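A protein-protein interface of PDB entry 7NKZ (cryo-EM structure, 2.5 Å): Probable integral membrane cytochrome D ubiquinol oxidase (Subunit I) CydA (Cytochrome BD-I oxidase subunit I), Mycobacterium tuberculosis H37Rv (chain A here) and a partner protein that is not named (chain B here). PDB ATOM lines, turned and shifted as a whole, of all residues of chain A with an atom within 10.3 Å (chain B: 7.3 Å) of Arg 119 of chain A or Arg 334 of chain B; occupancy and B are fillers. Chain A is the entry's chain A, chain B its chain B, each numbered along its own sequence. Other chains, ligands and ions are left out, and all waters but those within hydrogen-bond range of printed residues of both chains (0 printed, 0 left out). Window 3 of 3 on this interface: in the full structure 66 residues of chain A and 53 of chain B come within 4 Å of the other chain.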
ATOM      1  N   GLY A 111      23.186 -17.266  -2.332  1.00  0.00           N
ATOM      2  CA  GLY A 111      22.090 -17.959  -2.983  1.00  0.00           C
ATOM      3  C   GLY A 111      20.810 -17.150  -3.004  1.00  0.00           C
ATOM      4  O   GLY A 111      20.048 -17.214  -3.973  1.00  0.00           O
ATOM      5  N   LEU A 112      20.554 -16.385  -1.941  1.00  0.00           N
ATOM      6  CA  LEU A 112      19.394 -15.502  -1.924  1.00  0.00           C
ATOM      7  C   LEU A 112      19.516 -14.396  -2.963  1.00  0.00           C
ATOM      8  O   LEU A 112      18.513 -13.998  -3.563  1.00  0.00           O
ATOM      9  CB  LEU A 112      19.211 -14.900  -0.531  1.00  0.00           C
ATOM     10  CG  LEU A 112      18.863 -15.869   0.598  1.00  0.00           C
ATOM     11  CD1 LEU A 112      19.065 -15.209   1.951  1.00  0.00           C
ATOM     12  CD2 LEU A 112      17.433 -16.358   0.453  1.00  0.00           C
ATOM     13  N   TRP A 113      20.729 -13.887  -3.186  1.00  0.00           N
ATOM     14  CA  TRP A 113      20.926 -12.831  -4.171  1.00  0.00           C
ATOM     15  C   TRP A 113      20.773 -13.340  -5.599  1.00  0.00           C
ATOM     16  O   TRP A 113      20.259 -12.615  -6.458  1.00  0.00           O
ATOM     17  CB  TRP A 113      22.305 -12.194  -3.983  1.00  0.00           C
ATOM     18  CG  TRP A 113      22.564 -11.033  -4.891  1.00  0.00           C
ATOM     19  CD1 TRP A 113      22.012  -9.788  -4.808  1.00  0.00           C
ATOM     20  CD2 TRP A 113      23.452 -11.003  -6.015  1.00  0.00           C
ATOM     21  NE1 TRP A 113      22.495  -8.988  -5.813  1.00  0.00           N
ATOM     22  CE2 TRP A 113      23.382  -9.710  -6.568  1.00  0.00           C
ATOM     23  CE3 TRP A 113      24.297 -11.947  -6.608  1.00  0.00           C
ATOM     24  CZ2 TRP A 113      24.125  -9.335  -7.685  1.00  0.00           C
ATOM     25  CZ3 TRP A 113      25.034 -11.573  -7.717  1.00  0.00           C
ATOM     26  CH2 TRP A 113      24.943 -10.278  -8.244  1.00  0.00           C
ATOM     27  N   ILE A 114      21.211 -14.571  -5.873  1.00  0.00           N
ATOM     28  CA  ILE A 114      21.134 -15.104  -7.230  1.00  0.00           C
ATOM     29  C   ILE A 114      19.689 -15.412  -7.607  1.00  0.00           C
ATOM     30  O   ILE A 114      19.219 -15.035  -8.687  1.00  0.00           O
ATOM     31  CB  ILE A 114      22.027 -16.352  -7.365  1.00  0.00           C
ATOM     32  CG1 ILE A 114      23.498 -15.982  -7.170  1.00  0.00           C
ATOM     33  CG2 ILE A 114      21.822 -17.011  -8.720  1.00  0.00           C
ATOM     34  CD1 ILE A 114      24.421 -17.178  -7.108  1.00  0.00           C
ATOM     35  N   PHE A 115      18.963 -16.097  -6.723  1.00  0.00           N
ATOM     36  CA  PHE A 115      17.624 -16.590  -7.021  1.00  0.00           C
ATOM     37  C   PHE A 115      16.523 -15.734  -6.403  1.00  0.00           C
ATOM     38  O   PHE A 115      15.356 -16.138  -6.415  1.00  0.00           O
ATOM     39  CB  PHE A 115      17.482 -18.041  -6.555  1.00  0.00           C
ATOM     40  CG  PHE A 115      18.420 -18.995  -7.239  1.00  0.00           C
ATOM     41  CD1 PHE A 115      19.683 -19.238  -6.726  1.00  0.00           C
ATOM     42  CD2 PHE A 115      18.033 -19.656  -8.393  1.00  0.00           C
ATOM     43  CE1 PHE A 115      20.544 -20.119  -7.352  1.00  0.00           C
ATOM     44  CE2 PHE A 115      18.890 -20.538  -9.025  1.00  0.00           C
ATOM     45  CZ  PHE A 115      20.147 -20.769  -8.504  1.00  0.00           C
ATOM     46  N   GLY A 116      16.863 -14.566  -5.865  1.00  0.00           N
ATOM     47  CA  GLY A 116      15.869 -13.730  -5.220  1.00  0.00           C
ATOM     48  C   GLY A 116      15.602 -12.419  -5.926  1.00  0.00           C
ATOM     49  O   GLY A 116      15.114 -11.466  -5.309  1.00  0.00           O
ATOM     50  N   TRP A 117      15.922 -12.352  -7.220  1.00  0.00           N
ATOM     51  CA  TRP A 117      15.694 -11.122  -7.972  1.00  0.00           C
ATOM     52  C   TRP A 117      14.206 -10.815  -8.102  1.00  0.00           C
ATOM     53  O   TRP A 117      13.793  -9.658  -7.970  1.00  0.00           O
ATOM     54  CB  TRP A 117      16.346 -11.221  -9.350  1.00  0.00           C
ATOM     55  CG  TRP A 117      17.824 -10.994  -9.322  1.00  0.00           C
ATOM     56  CD1 TRP A 117      18.798 -11.947  -9.270  1.00  0.00           C
ATOM     57  CD2 TRP A 117      18.498  -9.731  -9.333  1.00  0.00           C
ATOM     58  NE1 TRP A 117      20.038 -11.355  -9.252  1.00  0.00           N
ATOM     59  CE2 TRP A 117      19.881  -9.994  -9.290  1.00  0.00           C
ATOM     60  CE3 TRP A 117      18.066  -8.401  -9.378  1.00  0.00           C
ATOM     61  CZ2 TRP A 117      20.835  -8.980  -9.290  1.00  0.00           C
ATOM     62  CZ3 TRP A 117      19.015  -7.395  -9.377  1.00  0.00           C
ATOM     63  CH2 TRP A 117      20.382  -7.691  -9.334  1.00  0.00           C
ATOM     64  N   ASN A 118      13.388 -11.835  -8.358  1.00  0.00           N
ATOM     65  CA  ASN A 118      11.953 -11.659  -8.522  1.00  0.00           C
ATOM     66  C   ASN A 118      11.143 -12.219  -7.362  1.00  0.00           C
ATOM     67  O   ASN A 118       9.912 -12.111  -7.376  1.00  0.00           O
ATOM     68  CB  ASN A 118      11.488 -12.304  -9.833  1.00  0.00           C
ATOM     69  CG  ASN A 118      12.116 -11.661 -11.054  1.00  0.00           C
ATOM     70  OD1 ASN A 118      12.403 -10.464 -11.059  1.00  0.00           O
ATOM     71  ND2 ASN A 118      12.334 -12.455 -12.095  1.00  0.00           N
ATOM     72  N   ARG A 119      11.792 -12.812  -6.362  1.00  0.00           N
ATOM     73  CA  ARG A 119      11.098 -13.374  -5.209  1.00  0.00           C
ATOM     74  C   ARG A 119      11.206 -12.503  -3.966  1.00  0.00           C
ATOM     75  O   ARG A 119      10.198 -12.263  -3.295  1.00  0.00           O
ATOM     76  CB  ARG A 119      11.639 -14.773  -4.897  1.00  0.00           C
ATOM     77  CG  ARG A 119      11.524 -15.755  -6.051  1.00  0.00           C
ATOM     78  CD  ARG A 119      11.739 -17.185  -5.586  1.00  0.00           C
ATOM     79  NE  ARG A 119      11.675 -18.134  -6.693  1.00  0.00           N
ATOM     80  CZ  ARG A 119      11.641 -19.455  -6.544  1.00  0.00           C
ATOM     81  NH1 ARG A 119      11.586 -20.242  -7.608  1.00  0.00           N
ATOM     82  NH2 ARG A 119      11.660 -19.988  -5.330  1.00  0.00           N
ATOM     83  N   LEU A 120      12.407 -12.024  -3.642  1.00  0.00           N
ATOM     84  CA  LEU A 120      12.610 -11.177  -2.478  1.00  0.00           C
ATOM     85  C   LEU A 120      12.284  -9.722  -2.804  1.00  0.00           C
ATOM     86  O   LEU A 120      12.382  -9.300  -3.961  1.00  0.00           O
ATOM     87  CB  LEU A 120      14.053 -11.278  -1.992  1.00  0.00           C
ATOM     88  CG  LEU A 120      14.512 -12.651  -1.495  1.00  0.00           C
ATOM     89  CD1 LEU A 120      15.994 -12.630  -1.156  1.00  0.00           C
ATOM     90  CD2 LEU A 120      13.690 -13.084  -0.292  1.00  0.00           C
ATOM     91  N   PRO A 121      11.887  -8.938  -1.802  1.00  0.00           N
ATOM     92  CA  PRO A 121      11.671  -7.505  -2.031  1.00  0.00           C
ATOM     93  C   PRO A 121      12.976  -6.802  -2.376  1.00  0.00           C
ATOM     94  O   PRO A 121      14.071  -7.285  -2.083  1.00  0.00           O
ATOM     95  CB  PRO A 121      11.105  -7.008  -0.695  1.00  0.00           C
ATOM     96  CG  PRO A 121      10.575  -8.234  -0.022  1.00  0.00           C
ATOM     97  CD  PRO A 121      11.478  -9.348  -0.449  1.00  0.00           C
ATOM     98  N   ARG A 122      12.842  -5.639  -3.019  1.00  0.00           N
ATOM     99  CA  ARG A 122      14.018  -4.893  -3.455  1.00  0.00           C
ATOM    100  C   ARG A 122      14.904  -4.498  -2.281  1.00  0.00           C
ATOM    101  O   ARG A 122      16.133  -4.609  -2.368  1.00  0.00           O
ATOM    102  CB  ARG A 122      13.595  -3.651  -4.238  1.00  0.00           C
ATOM    103  CG  ARG A 122      12.830  -3.953  -5.516  1.00  0.00           C
ATOM    104  CD  ARG A 122      13.199  -2.978  -6.623  1.00  0.00           C
ATOM    105  NE  ARG A 122      13.277  -1.603  -6.136  1.00  0.00           N
ATOM    106  CZ  ARG A 122      13.755  -0.585  -6.845  1.00  0.00           C
ATOM    107  NH1 ARG A 122      14.202  -0.785  -8.077  1.00  0.00           N
ATOM    108  NH2 ARG A 122      13.786   0.633  -6.321  1.00  0.00           N
ATOM    109  N   LEU A 123      14.308  -4.032  -1.181  1.00  0.00           N
ATOM    110  CA  LEU A 123      15.098  -3.693  -0.002  1.00  0.00           C
ATOM    111  C   LEU A 123      15.750  -4.925   0.613  1.00  0.00           C
ATOM    112  O   LEU A 123      16.911  -4.865   1.033  1.00  0.00           O
ATOM    113  CB  LEU A 123      14.225  -2.981   1.030  1.00  0.00           C
ATOM    114  CG  LEU A 123      13.929  -1.499   0.785  1.00  0.00           C
ATOM    115  CD1 LEU A 123      13.692  -0.776   2.101  1.00  0.00           C
ATOM    116  CD2 LEU A 123      15.056  -0.836   0.004  1.00  0.00           C
ATOM    117  N   VAL A 124      15.024  -6.042   0.681  1.00  0.00           N
ATOM    118  CA  VAL A 124      15.587  -7.264   1.247  1.00  0.00           C
ATOM    119  C   VAL A 124      16.655  -7.844   0.329  1.00  0.00           C
ATOM    120  O   VAL A 124      17.706  -8.300   0.794  1.00  0.00           O
ATOM    121  CB  VAL A 124      14.466  -8.281   1.531  1.00  0.00           C
ATOM    122  CG1 VAL A 124      15.033  -9.525   2.198  1.00  0.00           C
ATOM    123  CG2 VAL A 124      13.387  -7.650   2.397  1.00  0.00           C
ATOM    124  N   HIS A 125      16.406  -7.842  -0.983  1.00  0.00           N
ATOM    125  CA  HIS A 125      17.391  -8.365  -1.923  1.00  0.00           C
ATOM    126  C   HIS A 125      18.648  -7.504  -1.958  1.00  0.00           C
ATOM    127  O   HIS A 125      19.750  -8.028  -2.153  1.00  0.00           O
ATOM    128  CB  HIS A 125      16.780  -8.472  -3.320  1.00  0.00           C
ATOM    129  CG  HIS A 125      17.672  -9.135  -4.322  1.00  0.00           C
ATOM    130  ND1 HIS A 125      18.254  -8.452  -5.367  1.00  0.00           N
ATOM    131  CD2 HIS A 125      18.079 -10.421  -4.439  1.00  0.00           C
ATOM    132  CE1 HIS A 125      18.983  -9.287  -6.086  1.00  0.00           C
ATOM    133  NE2 HIS A 125      18.894 -10.489  -5.544  1.00  0.00           N
ATOM    134  N   LEU A 126      18.503  -6.188  -1.778  1.00  0.00           N
ATOM    135  CA  LEU A 126      19.670  -5.316  -1.713  1.00  0.00           C
ATOM    136  C   LEU A 126      20.540  -5.632  -0.503  1.00  0.00           C
ATOM    137  O   LEU A 126      21.771  -5.607  -0.603  1.00  0.00           O
ATOM    138  CB  LEU A 126      19.232  -3.852  -1.686  1.00  0.00           C
ATOM    139  CG  LEU A 126      20.340  -2.804  -1.557  1.00  0.00           C
ATOM    140  CD1 LEU A 126      21.329  -2.922  -2.704  1.00  0.00           C
ATOM    141  CD2 LEU A 126      19.750  -1.405  -1.495  1.00  0.00           C
ATOM    142  N   CYS A 128      20.929  -8.500   0.821  1.00  0.00           N
ATOM    143  CA  CYS A 128      21.589  -9.789   0.637  1.00  0.00           C
ATOM    144  C   CYS A 128      22.988  -9.622   0.054  1.00  0.00           C
ATOM    145  O   CYS A 128      23.934 -10.278   0.503  1.00  0.00           O
ATOM    146  CB  CYS A 128      20.739 -10.692  -0.256  1.00  0.00           C
ATOM    147  SG  CYS A 128      19.171 -11.209   0.480  1.00  0.00           S
ATOM    148  N   THR B  49      15.811 -29.216 -13.382  1.00  0.00           N
ATOM    149  CA  THR B  49      14.801 -29.109 -12.333  1.00  0.00           C
ATOM    150  C   THR B  49      15.325 -29.642 -11.005  1.00  0.00           C
ATOM    151  O   THR B  49      15.106 -29.029  -9.953  1.00  0.00           O
ATOM    152  CB  THR B  49      13.533 -29.855 -12.748  1.00  0.00           C
ATOM    153  OG1 THR B  49      13.064 -29.345 -14.001  1.00  0.00           O
ATOM    154  CG2 THR B  49      12.444 -29.681 -11.700  1.00  0.00           C
ATOM    155  N   ASN B  52      18.098 -27.186  -9.591  1.00  0.00           N
ATOM    156  CA  ASN B  52      17.585 -25.946  -9.019  1.00  0.00           C
ATOM    157  C   ASN B  52      16.966 -26.137  -7.641  1.00  0.00           C
ATOM    158  O   ASN B  52      16.779 -25.147  -6.926  1.00  0.00           O
ATOM    159  CB  ASN B  52      16.559 -25.317  -9.964  1.00  0.00           C
ATOM    160  CG  ASN B  52      17.191 -24.783 -11.234  1.00  0.00           C
ATOM    161  OD1 ASN B  52      18.413 -24.772 -11.377  1.00  0.00           O
ATOM    162  ND2 ASN B  52      16.358 -24.334 -12.165  1.00  0.00           N
ATOM    163  N   PRO B  56      19.958 -22.481  -4.544  1.00  0.00           N
ATOM    164  CA  PRO B  56      20.320 -21.411  -3.608  1.00  0.00           C
ATOM    165  C   PRO B  56      20.710 -21.879  -2.214  1.00  0.00           C
ATOM    166  O   PRO B  56      20.811 -21.042  -1.315  1.00  0.00           O
ATOM    167  CB  PRO B  56      19.034 -20.572  -3.552  1.00  0.00           C
ATOM    168  CG  PRO B  56      17.952 -21.560  -3.770  1.00  0.00           C
ATOM    169  CD  PRO B  56      18.499 -22.573  -4.739  1.00  0.00           C
ATOM    170  N   LYS B 188      10.320 -30.984  -3.219  1.00  0.00           N
ATOM    171  CA  LYS B 188      10.644 -29.691  -3.805  1.00  0.00           C
ATOM    172  C   LYS B 188      10.206 -29.563  -5.258  1.00  0.00           C
ATOM    173  O   LYS B 188      10.425 -28.510  -5.864  1.00  0.00           O
ATOM    174  CB  LYS B 188      12.152 -29.431  -3.701  1.00  0.00           C
ATOM    175  CG  LYS B 188      12.671 -29.350  -2.276  1.00  0.00           C
ATOM    176  CD  LYS B 188      12.334 -28.014  -1.638  1.00  0.00           C
ATOM    177  CE  LYS B 188      13.057 -26.875  -2.337  1.00  0.00           C
ATOM    178  NZ  LYS B 188      12.810 -25.568  -1.670  1.00  0.00           N
ATOM    179  N   SER B 190       7.092 -30.821  -8.440  1.00  0.00           N
ATOM    180  CA  SER B 190       5.741 -31.289  -8.703  1.00  0.00           C
ATOM    181  C   SER B 190       5.607 -31.610 -10.182  1.00  0.00           C
ATOM    182  O   SER B 190       6.202 -30.943 -11.034  1.00  0.00           O
ATOM    183  CB  SER B 190       4.692 -30.249  -8.286  1.00  0.00           C
ATOM    184  OG  SER B 190       4.872 -29.034  -8.993  1.00  0.00           O
ATOM    185  N   VAL B 325      12.005 -19.279   1.919  1.00  0.00           N
ATOM    186  CA  VAL B 325      11.835 -18.402   0.765  1.00  0.00           C
ATOM    187  C   VAL B 325      11.609 -19.221  -0.501  1.00  0.00           C
ATOM    188  O   VAL B 325      10.719 -18.914  -1.303  1.00  0.00           O
ATOM    189  CB  VAL B 325      13.048 -17.464   0.625  1.00  0.00           C
ATOM    190  CG1 VAL B 325      13.021 -16.753  -0.718  1.00  0.00           C
ATOM    191  CG2 VAL B 325      13.070 -16.457   1.764  1.00  0.00           C
ATOM    192  N   PHE B 326      12.400 -20.275  -0.697  1.00  0.00           N
ATOM    193  CA  PHE B 326      12.290 -21.138  -1.865  1.00  0.00           C
ATOM    194  C   PHE B 326      11.515 -22.418  -1.569  1.00  0.00           C
ATOM    195  O   PHE B 326      11.801 -23.469  -2.153  1.00  0.00           O
ATOM    196  CB  PHE B 326      13.680 -21.472  -2.408  1.00  0.00           C
ATOM    197  CG  PHE B 326      14.563 -20.271  -2.585  1.00  0.00           C
ATOM    198  CD1 PHE B 326      14.400 -19.430  -3.674  1.00  0.00           C
ATOM    199  CD2 PHE B 326      15.556 -19.983  -1.666  1.00  0.00           C
ATOM    200  CE1 PHE B 326      15.210 -18.323  -3.839  1.00  0.00           C
ATOM    201  CE2 PHE B 326      16.370 -18.879  -1.827  1.00  0.00           C
ATOM    202  CZ  PHE B 326      16.197 -18.048  -2.914  1.00  0.00           C
ATOM    203  N   ARG B 327      10.532 -22.350  -0.667  1.00  0.00           N
ATOM    204  CA  ARG B 327       9.752 -23.530  -0.321  1.00  0.00           C
ATOM    205  C   ARG B 327       8.797 -23.945  -1.433  1.00  0.00           C
ATOM    206  O   ARG B 327       8.318 -25.083  -1.427  1.00  0.00           O
ATOM    207  CB  ARG B 327       8.961 -23.281   0.965  1.00  0.00           C
ATOM    208  CG  ARG B 327       7.798 -22.318   0.793  1.00  0.00           C
ATOM    209  CD  ARG B 327       7.157 -21.972   2.126  1.00  0.00           C
ATOM    210  NE  ARG B 327       5.980 -21.125   1.961  1.00  0.00           N
ATOM    211  CZ  ARG B 327       6.023 -19.806   1.811  1.00  0.00           C
ATOM    212  NH1 ARG B 327       7.188 -19.174   1.806  1.00  0.00           N
ATOM    213  NH2 ARG B 327       4.900 -19.116   1.668  1.00  0.00           N
ATOM    214  N   GLN B 328       8.512 -23.053  -2.379  1.00  0.00           N
ATOM    215  CA  GLN B 328       7.586 -23.374  -3.455  1.00  0.00           C
ATOM    216  C   GLN B 328       8.172 -24.446  -4.366  1.00  0.00           C
ATOM    217  O   GLN B 328       9.350 -24.402  -4.729  1.00  0.00           O
ATOM    218  CB  GLN B 328       7.257 -22.119  -4.263  1.00  0.00           C
ATOM    219  CG  GLN B 328       6.188 -22.323  -5.323  1.00  0.00           C
ATOM    220  CD  GLN B 328       5.875 -21.052  -6.088  1.00  0.00           C
ATOM    221  OE1 GLN B 328       6.539 -20.030  -5.913  1.00  0.00           O
ATOM    222  NE2 GLN B 328       4.860 -21.108  -6.942  1.00  0.00           N
ATOM    223  N   ARG B 329       7.338 -25.415  -4.734  1.00  0.00           N
ATOM    224  CA  ARG B 329       7.778 -26.483  -5.618  1.00  0.00           C
ATOM    225  C   ARG B 329       8.004 -25.950  -7.027  1.00  0.00           C
ATOM    226  O   ARG B 329       7.261 -25.091  -7.511  1.00  0.00           O
ATOM    227  CB  ARG B 329       6.749 -27.612  -5.642  1.00  0.00           C
ATOM    228  CG  ARG B 329       6.503 -28.258  -4.289  1.00  0.00           C
ATOM    229  CD  ARG B 329       5.426 -29.327  -4.379  1.00  0.00           C
ATOM    230  NE  ARG B 329       5.139 -29.926  -3.079  1.00  0.00           N
ATOM    231  CZ  ARG B 329       5.307 -31.214  -2.798  1.00  0.00           C
ATOM    232  NH1 ARG B 329       5.762 -32.044  -3.725  1.00  0.00           N
ATOM    233  NH2 ARG B 329       5.019 -31.673  -1.588  1.00  0.00           N
ATOM    234  N   ILE B 330       9.036 -26.466  -7.686  1.00  0.00           N
ATOM    235  CA  ILE B 330       9.388 -26.070  -9.045  1.00  0.00           C
ATOM    236  C   ILE B 330       9.079 -27.237  -9.975  1.00  0.00           C
ATOM    237  O   ILE B 330       9.363 -28.396  -9.650  1.00  0.00           O
ATOM    238  CB  ILE B 330      10.859 -25.632  -9.150  1.00  0.00           C
ATOM    239  CG1 ILE B 330      11.809 -26.798  -8.856  1.00  0.00           C
ATOM    240  CG2 ILE B 330      11.131 -24.463  -8.213  1.00  0.00           C
ATOM    241  CD1 ILE B 330      13.231 -26.372  -8.553  1.00  0.00           C
ATOM    242  N   SER B 331       8.464 -26.933 -11.113  1.00  0.00           N
ATOM    243  CA  SER B 331       8.112 -27.932 -12.106  1.00  0.00           C
ATOM    244  C   SER B 331       8.902 -27.692 -13.388  1.00  0.00           C
ATOM    245  O   SER B 331       9.760 -26.810 -13.469  1.00  0.00           O
ATOM    246  CB  SER B 331       6.604 -27.913 -12.370  1.00  0.00           C
ATOM    247  OG  SER B 331       6.186 -26.642 -12.838  1.00  0.00           O
ATOM    248  N   ALA B 332       8.606 -28.499 -14.411  1.00  0.00           N
ATOM    249  CA  ALA B 332       9.262 -28.334 -15.701  1.00  0.00           C
ATOM    250  C   ALA B 332       8.851 -27.044 -16.397  1.00  0.00           C
ATOM    251  O   ALA B 332       9.658 -26.470 -17.137  1.00  0.00           O
ATOM    252  CB  ALA B 332       8.961 -29.532 -16.602  1.00  0.00           C
ATOM    253  N   GLU B 333       7.622 -26.575 -16.178  1.00  0.00           N
ATOM    254  CA  GLU B 333       7.167 -25.334 -16.791  1.00  0.00           C
ATOM    255  C   GLU B 333       7.712 -24.097 -16.089  1.00  0.00           C
ATOM    256  O   GLU B 333       7.700 -23.012 -16.679  1.00  0.00           O
ATOM    257  CB  GLU B 333       5.637 -25.280 -16.807  1.00  0.00           C
ATOM    258  CG  GLU B 333       4.982 -26.292 -17.735  1.00  0.00           C
ATOM    259  CD  GLU B 333       4.880 -27.675 -17.118  1.00  0.00           C
ATOM    260  OE1 GLU B 333       5.114 -27.802 -15.899  1.00  0.00           O
ATOM    261  OE2 GLU B 333       4.567 -28.634 -17.855  1.00  0.00           O
ATOM    262  N   ARG B 334       8.186 -24.234 -14.852  1.00  0.00           N
ATOM    263  CA  ARG B 334       8.755 -23.115 -14.114  1.00  0.00           C
ATOM    264  C   ARG B 334      10.239 -22.915 -14.386  1.00  0.00           C
ATOM    265  O   ARG B 334      10.804 -21.910 -13.939  1.00  0.00           O
ATOM    266  CB  ARG B 334       8.537 -23.307 -12.609  1.00  0.00           C
ATOM    267  CG  ARG B 334       7.439 -22.436 -12.023  1.00  0.00           C
ATOM    268  CD  ARG B 334       6.952 -22.983 -10.690  1.00  0.00           C
ATOM    269  NE  ARG B 334       7.810 -22.578  -9.580  1.00  0.00           N
ATOM    270  CZ  ARG B 334       7.831 -21.358  -9.050  1.00  0.00           C
ATOM    271  NH1 ARG B 334       7.034 -20.410  -9.524  1.00  0.00           N
ATOM    272  NH2 ARG B 334       8.648 -21.087  -8.042  1.00  0.00           N
ATOM    273  N   ILE B 335      10.879 -23.837 -15.096  1.00  0.00           N
ATOM    274  CA  ILE B 335      12.302 -23.734 -15.405  1.00  0.00           C
ATOM    275  C   ILE B 335      12.493 -22.687 -16.497  1.00  0.00           C
ATOM    276  O   ILE B 335      11.879 -22.793 -17.568  1.00  0.00           O
ATOM    277  CB  ILE B 335      12.881 -25.092 -15.832  1.00  0.00           C
ATOM    278  CG1 ILE B 335      12.795 -26.093 -14.678  1.00  0.00           C
ATOM    279  CG2 ILE B 335      14.320 -24.935 -16.294  1.00  0.00           C
ATOM    280  CD1 ILE B 335      13.580 -25.682 -13.454  1.00  0.00           C
ATOM    281  N   PRO B 336      13.318 -21.670 -16.274  1.00  0.00           N
ATOM    282  CA  PRO B 336      13.556 -20.661 -17.310  1.00  0.00           C
ATOM    283  C   PRO B 336      14.330 -21.253 -18.475  1.00  0.00           C
ATOM    284  O   PRO B 336      15.038 -22.258 -18.311  1.00  0.00           O
ATOM    285  CB  PRO B 336      14.378 -19.590 -16.579  1.00  0.00           C
ATOM    286  CG  PRO B 336      15.052 -20.329 -15.474  1.00  0.00           C
ATOM    287  CD  PRO B 336      14.082 -21.395 -15.044  1.00  0.00           C
ATOM    288  N   PRO B 337      14.209 -20.669 -19.670  1.00  0.00           N
ATOM    289  CA  PRO B 337      14.975 -21.175 -20.806  1.00  0.00           C
ATOM    290  C   PRO B 337      16.465 -21.022 -20.561  1.00  0.00           C
ATOM    291  O   PRO B 337      16.902 -20.090 -19.863  1.00  0.00           O
ATOM    292  CB  PRO B 337      14.504 -20.291 -21.974  1.00  0.00           C
ATOM    293  CG  PRO B 337      13.959 -19.061 -21.327  1.00  0.00           C
ATOM    294  CD  PRO B 337      13.357 -19.526 -20.038  1.00  0.00           C
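NH1 of Arg 119 of chain A sits close to NH2 of Arg 334 of chain B, at 3.1 Å.
OE1 of Gln 328 of chain B sits at hydrogen-bond distance from NH2 of Arg 334 of chain B (3.2 Å). The backbone carbonyl oxygen (O) of Arg 329 of chain B is in hydrogen-bond range of the guanidinium group (NE) of Arg 334 of chain B, at 3.3 Å.
Gly 111 of chain A touches Pro 56 of chain B (O to CB, 3.5 Å). Phe 326 of chain B touches Leu 112 of chain A. Phe 115 of chain A touches Pro 56 of chain B (CD1 to CB, 3.5 Å). Phe 326 of chain B touches Phe 115 of chain A (CE1 to O, 3.4 Å). Arg 119 of chain A touches Phe 326 of chain B. Val 325 of chain B touches Leu 120 of chain A.
Arg 119 of chain A touches two residues of chain B. Of chain A, only Arg 119 comes within 4 Å of Arg 334 of chain B. Of the printed residues of chain A, Phe 326 of chain B touches Leu 112 (3.6 Å), Phe 115 (3.4 Å) and Arg 119 (3.2 Å). No residue of chain A comes within 4 Å of Gln 328 of chain B. No residue of chain A comes within 4 Å of Ala 332 of chain B. No residue of chain A comes within 4 Å of Ile 335 of chain B. Of the printed residues of chain A, Val 325 of chain B touches Leu 120 (3.8 Å). Of the printed residues of chain A, Pro 56 of chain B touches Gly 111 and Phe 115. Of the printed residues of chain B, Phe 115 of chain A touches Pro 56 (3.5 Å) and Phe 326 (3.4 Å). Of the printed residues of chain B, Leu 120 of chain A touches Val 325. Of the printed residues of chain B, Leu 112 of chain A touches Phe 326. The nearest printed residue of chain A that does not touch Val 325 of chain B is Arg 119 of chain A (4.3 Å).
Printed residues of chain A that touch a printed residue of chain B: Gly 111, Leu 112, Phe 115, Arg 119 and Leu 120. Of the 18 printed residues of chain B, 4 touch a printed residue of chain A. Hydrophobic or aromatic side chains of chain B within 4 Å of the printed part of chain A: Pro 56, Val 325 and Phe 326. Among the printed residues, no Asp or Glu carboxylate lies within 4 Å of a Lys or Arg side-chain nitrogen of the other chain.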
